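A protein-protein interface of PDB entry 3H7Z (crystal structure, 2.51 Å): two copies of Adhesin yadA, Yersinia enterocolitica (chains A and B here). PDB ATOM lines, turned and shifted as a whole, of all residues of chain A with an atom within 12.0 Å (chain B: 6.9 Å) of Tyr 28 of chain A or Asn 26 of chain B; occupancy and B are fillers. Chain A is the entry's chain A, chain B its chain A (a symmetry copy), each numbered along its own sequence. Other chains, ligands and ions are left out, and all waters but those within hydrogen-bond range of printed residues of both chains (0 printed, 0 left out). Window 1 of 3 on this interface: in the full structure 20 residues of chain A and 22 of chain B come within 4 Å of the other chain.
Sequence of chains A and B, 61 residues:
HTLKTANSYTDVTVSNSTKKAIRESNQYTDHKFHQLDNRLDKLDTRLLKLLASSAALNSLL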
ATOM      1  N   THR A  18     -11.893 -29.433   9.565  1.00  0.00           N
ATOM      2  CA  THR A  18     -13.222 -29.376   9.046  1.00  0.00           C
ATOM      3  C   THR A  18     -13.859 -28.178   9.787  1.00  0.00           C
ATOM      4  O   THR A  18     -14.030 -27.115   9.205  1.00  0.00           O
ATOM      5  CB  THR A  18     -13.938 -30.706   9.299  1.00  0.00           C
ATOM      6  OG1 THR A  18     -13.228 -31.745   8.622  1.00  0.00           O
ATOM      7  CG2 THR A  18     -15.395 -30.685   8.805  1.00  0.00           C
ATOM      8  N   LYS A  19     -14.112 -28.337  11.086  1.00  0.00           N
ATOM      9  CA  LYS A  19     -14.605 -27.279  11.971  1.00  0.00           C
ATOM     10  C   LYS A  19     -14.154 -25.850  11.660  1.00  0.00           C
ATOM     11  O   LYS A  19     -14.919 -24.922  11.850  1.00  0.00           O
ATOM     12  CB  LYS A  19     -14.253 -27.586  13.435  1.00  0.00           C
ATOM     13  CG  LYS A  19     -15.205 -28.525  14.137  1.00  0.00           C
ATOM     14  CD  LYS A  19     -15.314 -28.197  15.653  1.00  0.00           C
ATOM     15  CE  LYS A  19     -16.662 -28.715  16.240  1.00  0.00           C
ATOM     16  NZ  LYS A  19     -17.027 -28.194  17.617  1.00  0.00           N
ATOM     17  N   LYS A  20     -12.918 -25.675  11.211  1.00  0.00           N
ATOM     18  CA  LYS A  20     -12.324 -24.336  11.015  1.00  0.00           C
ATOM     19  C   LYS A  20     -12.750 -23.736   9.690  1.00  0.00           C
ATOM     20  O   LYS A  20     -13.219 -22.602   9.655  1.00  0.00           O
ATOM     21  CB  LYS A  20     -10.792 -24.378  11.165  1.00  0.00           C
ATOM     22  CG  LYS A  20      -9.993 -23.241  10.525  1.00  0.00           C
ATOM     23  CD  LYS A  20      -8.859 -22.796  11.446  1.00  0.00           C
ATOM     24  CE  LYS A  20      -7.926 -21.802  10.787  1.00  0.00           C
ATOM     25  NZ  LYS A  20      -6.670 -21.639  11.610  1.00  0.00           N
ATOM     26  N   ALA A  21     -12.596 -24.518   8.622  1.00  0.00           N
ATOM     27  CA  ALA A  21     -13.076 -24.182   7.289  1.00  0.00           C
ATOM     28  C   ALA A  21     -14.564 -23.850   7.290  1.00  0.00           C
ATOM     29  O   ALA A  21     -14.989 -22.927   6.621  1.00  0.00           O
ATOM     30  CB  ALA A  21     -12.812 -25.317   6.335  1.00  0.00           C
ATOM     31  N   ILE A  22     -15.352 -24.615   8.018  1.00  0.00           N
ATOM     32  CA  ILE A  22     -16.746 -24.315   8.140  1.00  0.00           C
ATOM     33  C   ILE A  22     -16.893 -22.953   8.823  1.00  0.00           C
ATOM     34  O   ILE A  22     -17.136 -21.972   8.143  1.00  0.00           O
ATOM     35  CB  ILE A  22     -17.490 -25.448   8.824  1.00  0.00           C
ATOM     36  CG1 ILE A  22     -17.631 -26.615   7.841  1.00  0.00           C
ATOM     37  CG2 ILE A  22     -18.853 -24.999   9.266  1.00  0.00           C
ATOM     38  CD1 ILE A  22     -17.991 -27.943   8.472  1.00  0.00           C
ATOM     39  N   ARG A  23     -16.685 -22.869  10.135  1.00  0.00           N
ATOM     40  CA  ARG A  23     -16.726 -21.592  10.869  1.00  0.00           C
ATOM     41  C   ARG A  23     -16.326 -20.358  10.050  1.00  0.00           C
ATOM     42  O   ARG A  23     -16.939 -19.325  10.218  1.00  0.00           O
ATOM     43  CB  ARG A  23     -15.859 -21.662  12.143  1.00  0.00           C
ATOM     44  CG  ARG A  23     -16.063 -20.535  13.173  1.00  0.00           C
ATOM     45  CD  ARG A  23     -14.752 -19.960  13.736  1.00  0.00           C
ATOM     46  NE  ARG A  23     -13.967 -20.971  14.431  1.00  0.00           N
ATOM     47  CZ  ARG A  23     -12.688 -21.256  14.190  1.00  0.00           C
ATOM     48  NH1 ARG A  23     -12.002 -20.568  13.280  1.00  0.00           N
ATOM     49  NH2 ARG A  23     -12.085 -22.224  14.887  1.00  0.00           N
ATOM     50  N   GLU A  24     -15.312 -20.461   9.190  1.00  0.00           N
ATOM     51  CA  GLU A  24     -14.790 -19.298   8.451  1.00  0.00           C
ATOM     52  C   GLU A  24     -15.520 -19.025   7.144  1.00  0.00           C
ATOM     53  O   GLU A  24     -15.586 -17.884   6.681  1.00  0.00           O
ATOM     54  CB  GLU A  24     -13.288 -19.435   8.146  1.00  0.00           C
ATOM     55  CG  GLU A  24     -12.379 -18.820   9.209  1.00  0.00           C
ATOM     56  CD  GLU A  24     -10.892 -18.968   8.923  1.00  0.00           C
ATOM     57  OE1 GLU A  24     -10.403 -18.504   7.871  1.00  0.00           O
ATOM     58  OE2 GLU A  24     -10.195 -19.530   9.785  1.00  0.00           O
ATOM     59  N   SER A  25     -16.032 -20.088   6.543  1.00  0.00           N
ATOM     60  CA  SER A  25     -16.681 -20.004   5.263  1.00  0.00           C
ATOM     61  C   SER A  25     -18.136 -19.632   5.464  1.00  0.00           C
ATOM     62  O   SER A  25     -18.810 -19.227   4.520  1.00  0.00           O
ATOM     63  CB  SER A  25     -16.565 -21.335   4.547  1.00  0.00           C
ATOM     64  OG  SER A  25     -15.213 -21.605   4.252  1.00  0.00           O
ATOM     65  N   ASN A  26     -18.608 -19.814   6.693  1.00  0.00           N
ATOM     66  CA  ASN A  26     -19.893 -19.342   7.150  1.00  0.00           C
ATOM     67  C   ASN A  26     -19.773 -17.875   7.467  1.00  0.00           C
ATOM     68  O   ASN A  26     -20.601 -17.084   7.069  1.00  0.00           O
ATOM     69  CB  ASN A  26     -20.312 -20.093   8.403  1.00  0.00           C
ATOM     70  CG  ASN A  26     -20.815 -21.475   8.108  1.00  0.00           C
ATOM     71  OD1 ASN A  26     -20.661 -21.983   7.009  1.00  0.00           O
ATOM     72  ND2 ASN A  26     -21.446 -22.091   9.096  1.00  0.00           N
ATOM     73  N   GLN A  27     -18.708 -17.526   8.168  1.00  0.00           N
ATOM     74  CA  GLN A  27     -18.377 -16.152   8.525  1.00  0.00           C
ATOM     75  C   GLN A  27     -18.258 -15.168   7.368  1.00  0.00           C
ATOM     76  O   GLN A  27     -18.468 -13.988   7.558  1.00  0.00           O
ATOM     77  CB  GLN A  27     -17.058 -16.129   9.314  1.00  0.00           C
ATOM     78  CG  GLN A  27     -17.195 -16.378  10.815  1.00  0.00           C
ATOM     79  CD  GLN A  27     -15.950 -15.985  11.585  1.00  0.00           C
ATOM     80  OE1 GLN A  27     -15.965 -15.942  12.818  1.00  0.00           O
ATOM     81  NE2 GLN A  27     -14.870 -15.677  10.865  1.00  0.00           N
ATOM     82  N   TYR A  28     -17.854 -15.653   6.204  1.00  0.00           N
ATOM     83  CA  TYR A  28     -17.738 -14.835   4.990  1.00  0.00           C
ATOM     84  C   TYR A  28     -19.080 -14.813   4.249  1.00  0.00           C
ATOM     85  O   TYR A  28     -19.439 -13.830   3.615  1.00  0.00           O
ATOM     86  CB  TYR A  28     -16.632 -15.378   4.100  1.00  0.00           C
ATOM     87  CG  TYR A  28     -16.419 -14.700   2.759  1.00  0.00           C
ATOM     88  CD1 TYR A  28     -15.703 -13.493   2.637  1.00  0.00           C
ATOM     89  CD2 TYR A  28     -16.871 -15.301   1.592  1.00  0.00           C
ATOM     90  CE1 TYR A  28     -15.498 -12.890   1.385  1.00  0.00           C
ATOM     91  CE2 TYR A  28     -16.653 -14.719   0.349  1.00  0.00           C
ATOM     92  CZ  TYR A  28     -15.979 -13.527   0.255  1.00  0.00           C
ATOM     93  OH  TYR A  28     -15.812 -13.005  -1.006  1.00  0.00           O
ATOM     94  N   THR A  29     -19.823 -15.907   4.348  1.00  0.00           N
ATOM     95  CA  THR A  29     -21.185 -15.924   3.896  1.00  0.00           C
ATOM     96  C   THR A  29     -21.937 -14.849   4.673  1.00  0.00           C
ATOM     97  O   THR A  29     -22.711 -14.108   4.091  1.00  0.00           O
ATOM     98  CB  THR A  29     -21.823 -17.325   4.062  1.00  0.00           C
ATOM     99  OG1 THR A  29     -21.217 -18.227   3.126  1.00  0.00           O
ATOM    100  CG2 THR A  29     -23.351 -17.290   3.803  1.00  0.00           C
ATOM    101  N   ASP A  30     -21.679 -14.731   5.969  1.00  0.00           N
ATOM    102  CA  ASP A  30     -22.400 -13.766   6.784  1.00  0.00           C
ATOM    103  C   ASP A  30     -21.888 -12.344   6.622  1.00  0.00           C
ATOM    104  O   ASP A  30     -22.551 -11.398   7.011  1.00  0.00           O
ATOM    105  CB  ASP A  30     -22.397 -14.192   8.240  1.00  0.00           C
ATOM    106  CG  ASP A  30     -23.208 -15.442   8.472  1.00  0.00           C
ATOM    107  OD1 ASP A  30     -23.775 -15.999   7.517  1.00  0.00           O
ATOM    108  OD2 ASP A  30     -23.297 -15.884   9.627  1.00  0.00           O
ATOM    109  N   HIS A  31     -20.706 -12.196   6.042  1.00  0.00           N
ATOM    110  CA  HIS A  31     -20.174 -10.872   5.714  1.00  0.00           C
ATOM    111  C   HIS A  31     -21.007 -10.326   4.583  1.00  0.00           C
ATOM    112  O   HIS A  31     -21.553  -9.240   4.702  1.00  0.00           O
ATOM    113  CB  HIS A  31     -18.720 -10.986   5.268  1.00  0.00           C
ATOM    114  CG  HIS A  31     -18.087  -9.689   4.884  1.00  0.00           C
ATOM    115  ND1 HIS A  31     -17.988  -8.624   5.750  1.00  0.00           N
ATOM    116  CD2 HIS A  31     -17.469  -9.308   3.740  1.00  0.00           C
ATOM    117  CE1 HIS A  31     -17.348  -7.634   5.150  1.00  0.00           C
ATOM    118  NE2 HIS A  31     -17.028  -8.021   3.928  1.00  0.00           N
ATOM    119  N   LYS A  32     -21.105 -11.107   3.507  1.00  0.00           N
ATOM    120  CA  LYS A  32     -21.890 -10.766   2.331  1.00  0.00           C
ATOM    121  C   LYS A  32     -23.420 -11.018   2.443  1.00  0.00           C
ATOM    122  O   LYS A  32     -24.143 -10.656   1.549  1.00  0.00           O
ATOM    123  CB  LYS A  32     -21.313 -11.442   1.071  1.00  0.00           C
ATOM    124  CG  LYS A  32     -19.787 -11.417   0.906  1.00  0.00           C
ATOM    125  CD  LYS A  32     -19.222 -10.067   0.428  1.00  0.00           C
ATOM    126  CE  LYS A  32     -19.067  -9.955  -1.101  1.00  0.00           C
ATOM    127  NZ  LYS A  32     -18.233  -8.762  -1.505  1.00  0.00           N
ATOM    128  N   PHE A  33     -23.913 -11.631   3.516  1.00  0.00           N
ATOM    129  CA  PHE A  33     -25.348 -11.616   3.797  1.00  0.00           C
ATOM    130  C   PHE A  33     -25.665 -10.209   4.267  1.00  0.00           C
ATOM    131  O   PHE A  33     -26.450  -9.499   3.631  1.00  0.00           O
ATOM    132  CB  PHE A  33     -25.712 -12.633   4.882  1.00  0.00           C
ATOM    133  CG  PHE A  33     -27.139 -12.497   5.456  1.00  0.00           C
ATOM    134  CD1 PHE A  33     -28.207 -13.227   4.915  1.00  0.00           C
ATOM    135  CD2 PHE A  33     -27.392 -11.705   6.582  1.00  0.00           C
ATOM    136  CE1 PHE A  33     -29.497 -13.143   5.463  1.00  0.00           C
ATOM    137  CE2 PHE A  33     -28.673 -11.618   7.130  1.00  0.00           C
ATOM    138  CZ  PHE A  33     -29.726 -12.344   6.566  1.00  0.00           C
ATOM    139  N   HIS A  34     -25.025  -9.832   5.378  1.00  0.00           N
ATOM    140  CA  HIS A  34     -25.019  -8.485   5.958  1.00  0.00           C
ATOM    141  C   HIS A  34     -24.797  -7.368   4.931  1.00  0.00           C
ATOM    142  O   HIS A  34     -25.136  -6.225   5.199  1.00  0.00           O
ATOM    143  CB  HIS A  34     -23.894  -8.380   7.017  1.00  0.00           C
ATOM    144  CG  HIS A  34     -24.220  -8.977   8.364  1.00  0.00           C
ATOM    145  ND1 HIS A  34     -23.432  -8.758   9.476  1.00  0.00           N
ATOM    146  CD2 HIS A  34     -25.237  -9.771   8.782  1.00  0.00           C
ATOM    147  CE1 HIS A  34     -23.941  -9.397  10.515  1.00  0.00           C
ATOM    148  NE2 HIS A  34     -25.039 -10.019  10.122  1.00  0.00           N
ATOM    149  N   GLN A  35     -24.202  -7.675   3.784  1.00  0.00           N
ATOM    150  CA  GLN A  35     -23.882  -6.647   2.797  1.00  0.00           C
ATOM    151  C   GLN A  35     -24.930  -6.460   1.706  1.00  0.00           C
ATOM    152  O   GLN A  35     -24.974  -5.411   1.076  1.00  0.00           O
ATOM    153  CB  GLN A  35     -22.520  -6.901   2.163  1.00  0.00           C
ATOM    154  CG  GLN A  35     -21.385  -6.369   2.992  1.00  0.00           C
ATOM    155  CD  GLN A  35     -20.083  -6.215   2.226  1.00  0.00           C
ATOM    156  OE1 GLN A  35     -19.110  -5.657   2.749  1.00  0.00           O
ATOM    157  NE2 GLN A  35     -20.050  -6.706   0.993  1.00  0.00           N
ATOM    158  N   LEU A  36     -25.747  -7.475   1.455  1.00  0.00           N
ATOM    159  CA  LEU A  36     -26.828  -7.348   0.483  1.00  0.00           C
ATOM    160  C   LEU A  36     -28.176  -7.176   1.181  1.00  0.00           C
ATOM    161  O   LEU A  36     -29.094  -6.629   0.606  1.00  0.00           O
ATOM    162  CB  LEU A  36     -26.870  -8.548  -0.488  1.00  0.00           C
ATOM    163  CG  LEU A  36     -25.852  -8.687  -1.644  1.00  0.00           C
ATOM    164  CD1 LEU A  36     -26.096  -9.958  -2.435  1.00  0.00           C
ATOM    165  CD2 LEU A  36     -25.852  -7.507  -2.574  1.00  0.00           C
ATOM    166  N   ASP A  37     -28.261  -7.674   2.413  1.00  0.00           N
ATOM    167  CA  ASP A  37     -29.391  -7.523   3.333  1.00  0.00           C
ATOM    168  C   ASP A  37     -29.585  -6.031   3.629  1.00  0.00           C
ATOM    169  O   ASP A  37     -30.695  -5.583   3.884  1.00  0.00           O
ATOM    170  CB  ASP A  37     -29.052  -8.311   4.613  1.00  0.00           C
ATOM    171  CG  ASP A  37     -30.226  -8.477   5.585  1.00  0.00           C
ATOM    172  OD1 ASP A  37     -31.052  -9.399   5.419  1.00  0.00           O
ATOM    173  OD2 ASP A  37     -30.273  -7.738   6.589  1.00  0.00           O
ATOM    174  N   LYS B  20      -7.963 -24.605   1.259  1.00  0.00           N
ATOM    175  CA  LYS B  20      -8.617 -24.989  -0.009  1.00  0.00           C
ATOM    176  C   LYS B  20     -10.127 -24.920   0.111  1.00  0.00           C
ATOM    177  O   LYS B  20     -10.779 -24.299  -0.724  1.00  0.00           O
ATOM    178  CB  LYS B  20      -8.138 -26.371  -0.488  1.00  0.00           C
ATOM    179  CG  LYS B  20      -9.039 -27.126  -1.468  1.00  0.00           C
ATOM    180  CD  LYS B  20      -8.204 -27.803  -2.552  1.00  0.00           C
ATOM    181  CE  LYS B  20      -9.027 -28.712  -3.441  1.00  0.00           C
ATOM    182  NZ  LYS B  20      -8.121 -29.585  -4.278  1.00  0.00           N
ATOM    183  N   ALA B  21     -10.655 -25.545   1.162  1.00  0.00           N
ATOM    184  CA  ALA B  21     -12.062 -25.474   1.532  1.00  0.00           C
ATOM    185  C   ALA B  21     -12.534 -24.033   1.685  1.00  0.00           C
ATOM    186  O   ALA B  21     -13.627 -23.695   1.268  1.00  0.00           O
ATOM    187  CB  ALA B  21     -12.307 -26.226   2.812  1.00  0.00           C
ATOM    188  N   ILE B  22     -11.726 -23.196   2.304  1.00  0.00           N
ATOM    189  CA  ILE B  22     -12.060 -21.808   2.411  1.00  0.00           C
ATOM    190  C   ILE B  22     -12.127 -21.214   1.002  1.00  0.00           C
ATOM    191  O   ILE B  22     -13.217 -21.039   0.484  1.00  0.00           O
ATOM    192  CB  ILE B  22     -11.111 -21.090   3.355  1.00  0.00           C
ATOM    193  CG1 ILE B  22     -11.454 -21.481   4.796  1.00  0.00           C
ATOM    194  CG2 ILE B  22     -11.231 -19.602   3.198  1.00  0.00           C
ATOM    195  CD1 ILE B  22     -10.378 -21.171   5.815  1.00  0.00           C
ATOM    196  N   ARG B  23     -10.991 -20.967   0.357  1.00  0.00           N
ATOM    197  CA  ARG B  23     -10.952 -20.469  -1.030  1.00  0.00           C
ATOM    198  C   ARG B  23     -12.139 -20.892  -1.906  1.00  0.00           C
ATOM    199  O   ARG B  23     -12.600 -20.088  -2.689  1.00  0.00           O
ATOM    200  CB  ARG B  23      -9.635 -20.873  -1.723  1.00  0.00           C
ATOM    201  CG  ARG B  23      -9.308 -20.153  -3.045  1.00  0.00           C
ATOM    202  CD  ARG B  23      -8.803 -21.089  -4.157  1.00  0.00           C
ATOM    203  NE  ARG B  23      -7.571 -21.768  -3.781  1.00  0.00           N
ATOM    204  CZ  ARG B  23      -7.372 -23.085  -3.821  1.00  0.00           C
ATOM    205  NH1 ARG B  23      -8.324 -23.899  -4.270  1.00  0.00           N
ATOM    206  NH2 ARG B  23      -6.197 -23.586  -3.427  1.00  0.00           N
ATOM    207  N   GLU B  24     -12.613 -22.132  -1.784  1.00  0.00           N
ATOM    208  CA  GLU B  24     -13.671 -22.656  -2.666  1.00  0.00           C
ATOM    209  C   GLU B  24     -15.081 -22.356  -2.178  1.00  0.00           C
ATOM    210  O   GLU B  24     -16.018 -22.247  -2.973  1.00  0.00           O
ATOM    211  CB  GLU B  24     -13.547 -24.175  -2.876  1.00  0.00           C
ATOM    212  CG  GLU B  24     -12.717 -24.569  -4.097  1.00  0.00           C
ATOM    213  CD  GLU B  24     -12.574 -26.071  -4.301  1.00  0.00           C
ATOM    214  OE1 GLU B  24     -13.588 -26.786  -4.442  1.00  0.00           O
ATOM    215  OE2 GLU B  24     -11.423 -26.536  -4.354  1.00  0.00           O
ATOM    216  N   SER B  25     -15.221 -22.259  -0.865  1.00  0.00           N
ATOM    217  CA  SER B  25     -16.503 -22.058  -0.246  1.00  0.00           C
ATOM    218  C   SER B  25     -16.816 -20.575  -0.215  1.00  0.00           C
ATOM    219  O   SER B  25     -17.960 -20.185   0.001  1.00  0.00           O
ATOM    220  CB  SER B  25     -16.484 -22.628   1.158  1.00  0.00           C
ATOM    221  OG  SER B  25     -16.324 -24.028   1.105  1.00  0.00           O
ATOM    222  N   ASN B  26     -15.774 -19.769  -0.393  1.00  0.00           N
ATOM    223  CA  ASN B  26     -15.873 -18.343  -0.599  1.00  0.00           C
ATOM    224  C   ASN B  26     -16.248 -18.097  -2.037  1.00  0.00           C
ATOM    225  O   ASN B  26     -17.132 -17.319  -2.325  1.00  0.00           O
ATOM    226  CB  ASN B  26     -14.540 -17.676  -0.307  1.00  0.00           C
ATOM    227  CG  ASN B  26     -14.268 -17.544   1.162  1.00  0.00           C
ATOM    228  OD1 ASN B  26     -14.950 -18.132   1.987  1.00  0.00           O
ATOM    229  ND2 ASN B  26     -13.270 -16.743   1.502  1.00  0.00           N
ATOM    230  N   GLN B  27     -15.574 -18.800  -2.932  1.00  0.00           N
ATOM    231  CA  GLN B  27     -15.825 -18.753  -4.367  1.00  0.00           C
ATOM    232  C   GLN B  27     -17.247 -19.069  -4.809  1.00  0.00           C
ATOM    233  O   GLN B  27     -17.671 -18.608  -5.849  1.00  0.00           O
ATOM    234  CB  GLN B  27     -14.870 -19.719  -5.087  1.00  0.00           C
ATOM    235  CG  GLN B  27     -13.492 -19.147  -5.413  1.00  0.00           C
ATOM    236  CD  GLN B  27     -12.740 -19.986  -6.426  1.00  0.00           C
ATOM    237  OE1 GLN B  27     -11.700 -19.564  -6.940  1.00  0.00           O
ATOM    238  NE2 GLN B  27     -13.268 -21.170  -6.738  1.00  0.00           N
ATOM    239  N   TYR B  28     -17.941 -19.907  -4.055  1.00  0.00           N
ATOM    240  CA  TYR B  28     -19.338 -20.268  -4.330  1.00  0.00           C
ATOM    241  C   TYR B  28     -20.277 -19.258  -3.660  1.00  0.00           C
ATOM    242  O   TYR B  28     -21.351 -18.959  -4.163  1.00  0.00           O
ATOM    243  CB  TYR B  28     -19.617 -21.679  -3.840  1.00  0.00           C
ATOM    244  CG  TYR B  28     -21.039 -22.196  -3.973  1.00  0.00           C
ATOM    245  CD1 TYR B  28     -21.542 -22.692  -5.192  1.00  0.00           C
ATOM    246  CD2 TYR B  28     -21.866 -22.259  -2.861  1.00  0.00           C
ATOM    247  CE1 TYR B  28     -22.854 -23.185  -5.291  1.00  0.00           C
ATOM    248  CE2 TYR B  28     -23.157 -22.764  -2.948  1.00  0.00           C
ATOM    249  CZ  TYR B  28     -23.640 -23.216  -4.152  1.00  0.00           C
ATOM    250  OH  TYR B  28     -24.930 -23.690  -4.166  1.00  0.00           O
ATOM    251  N   THR B  29     -19.850 -18.724  -2.524  1.00  0.00           N
ATOM    252  CA  THR B  29     -20.526 -17.608  -1.926  1.00  0.00           C
ATOM    253  C   THR B  29     -20.512 -16.469  -2.941  1.00  0.00           C
ATOM    254  O   THR B  29     -21.520 -15.811  -3.130  1.00  0.00           O
ATOM    255  CB  THR B  29     -19.877 -17.203  -0.579  1.00  0.00           C
ATOM    256  OG1 THR B  29     -20.140 -18.227   0.389  1.00  0.00           O
ATOM    257  CG2 THR B  29     -20.446 -15.860  -0.054  1.00  0.00           C
ATOM    258  N   ASP B  30     -19.393 -16.268  -3.625  1.00  0.00           N
ATOM    259  CA  ASP B  30     -19.288 -15.165  -4.569  1.00  0.00           C
ATOM    260  C   ASP B  30     -19.970 -15.448  -5.897  1.00  0.00           C
ATOM    261  O   ASP B  30     -20.212 -14.541  -6.675  1.00  0.00           O
ATOM    262  CB  ASP B  30     -17.838 -14.769  -4.765  1.00  0.00           C
ATOM    263  CG  ASP B  30     -17.239 -14.155  -3.523  1.00  0.00           C
ATOM    264  OD1 ASP B  30     -17.929 -14.035  -2.498  1.00  0.00           O
ATOM    265  OD2 ASP B  30     -16.061 -13.774  -3.561  1.00  0.00           O
ATOM    266  N   HIS B  31     -20.282 -16.710  -6.153  1.00  0.00           N
ATOM    267  CA  HIS B  31     -21.057 -17.081  -7.338  1.00  0.00           C
ATOM    268  C   HIS B  31     -22.463 -16.580  -7.126  1.00  0.00           C
ATOM    269  O   HIS B  31     -22.977 -15.846  -7.956  1.00  0.00           O
ATOM    270  CB  HIS B  31     -21.076 -18.598  -7.499  1.00  0.00           C
ATOM    271  CG  HIS B  31     -21.865 -19.087  -8.669  1.00  0.00           C
ATOM    272  ND1 HIS B  31     -21.586 -18.713  -9.964  1.00  0.00           N
ATOM    273  CD2 HIS B  31     -22.893 -19.967  -8.741  1.00  0.00           C
ATOM    274  CE1 HIS B  31     -22.419 -19.332 -10.785  1.00  0.00           C
ATOM    275  NE2 HIS B  31     -23.226 -20.093 -10.067  1.00  0.00           N
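OG1 of Thr 29 of chain B sits at hydrogen-bond distance from OG1 of Thr 29 of chain A. The side-chain carboxylate of Asp 30 of chain B sits at hydrogen-bond distance from the side-chain hydroxyl of Tyr 28 of chain A.
The backbone carbonyl oxygen (O) of Ala 21 of chain A lies within hydrogen-bond range of the side-chain hydroxyl (OG) of Ser 25 of chain A. The backbone carbonyl oxygen of Ser 25 of chain A sits at hydrogen-bond distance from the side-chain hydroxyl of Thr 29 of chain A (3.0 Å). O of Ser 25 of chain B sits at hydrogen-bond distance from OG1 of Thr 29 of chain B. The backbone carbonyl oxygen (O) of Ala 21 of chain B sits at hydrogen-bond distance from the side-chain hydroxyl (OG) of Ser 25 of chain B, 2.7 Å away.
Ala 21 of chain A touches Ala 21 of chain B (CB to CB, 3.7 Å). OE1 of Glu 24 of chain A touches CD1 of Ile 22 of chain B, at 3.4 Å. Ala 21 of chain B touches Ser 25 of chain A (O to OG, 3.97 Å). OG of Ser 25 of chain A touches CA of Ile 22 of chain B, 3.7 Å away. Ser 25 of chain B touches Ser 25 of chain A. Asn 26 of chain B touches Tyr 28 of chain A (OD1 to CD2, 3.4 Å). Thr 29 of chain B touches Tyr 28 of chain A (CG2 to CD2, 3.98 Å).
Lys 19 of chain A touches none of the printed residues of chain B. Ile 22 of chain A touches none of the printed residues of chain B. Of the printed residues of chain B, Glu 24 of chain A touches Ile 22. Of chain B, only Asn 26, Thr 29 and Asp 30 come within 4 Å of Tyr 28 of chain A. Of the printed residues of chain B, Thr 29 of chain A touches Thr 29 (2.9 Å). Of the printed residues of chain A, Ala 21 of chain B touches Ala 21 (3.7 Å) and Ser 25 (3.97 Å). Of the printed residues of chain A, Ile 22 of chain B touches Glu 24 and Ser 25. Of the printed residues of chain A, Ser 25 of chain B touches Ser 25. Asn 26 of chain B touches just one residue of chain A: Tyr 28 (3.4 Å). Asp 30 of chain B touches just one residue of chain A: Tyr 28. The nearest residue of chain A that does not touch Asn 26 of chain B is Ser 25 of chain A (4.2 Å). The nearest printed residue of chain B that does not touch Thr 29 of chain A is Ser 25 of chain B (4.9 Å).
Hydrophobic or aromatic side chains of chain B within 4 Å of the printed part of chain A: Ala 21 and Ile 22. Of the 20 printed residues of chain A, 5 touch a printed residue of chain B. Among the printed residues, no Asp or Glu carboxylate lies within 4 Å of a Lys or Arg side-chain nitrogen of the other chain.
Ala 21 of chain A touches its own counterpart, Ala 21 of chain B. Ser 25 of chain B touches its own counterpart, Ser 25 of chain A. Tyr 28 of chain A touches Asn 26 of chain B, but with the chains exchanged Asn 26 of chain A does not touch Tyr 28 of chain B (9.9 Å). Tyr 28 of chain A touches Asp 30 of chain B, but with the chains exchanged Asp 30 of chain A does not touch Tyr 28 of chain B (10.7 Å). Of the 9 pairs that touch across the chains among the printed residues, 3 have their exchanged pair printed and touching as well.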
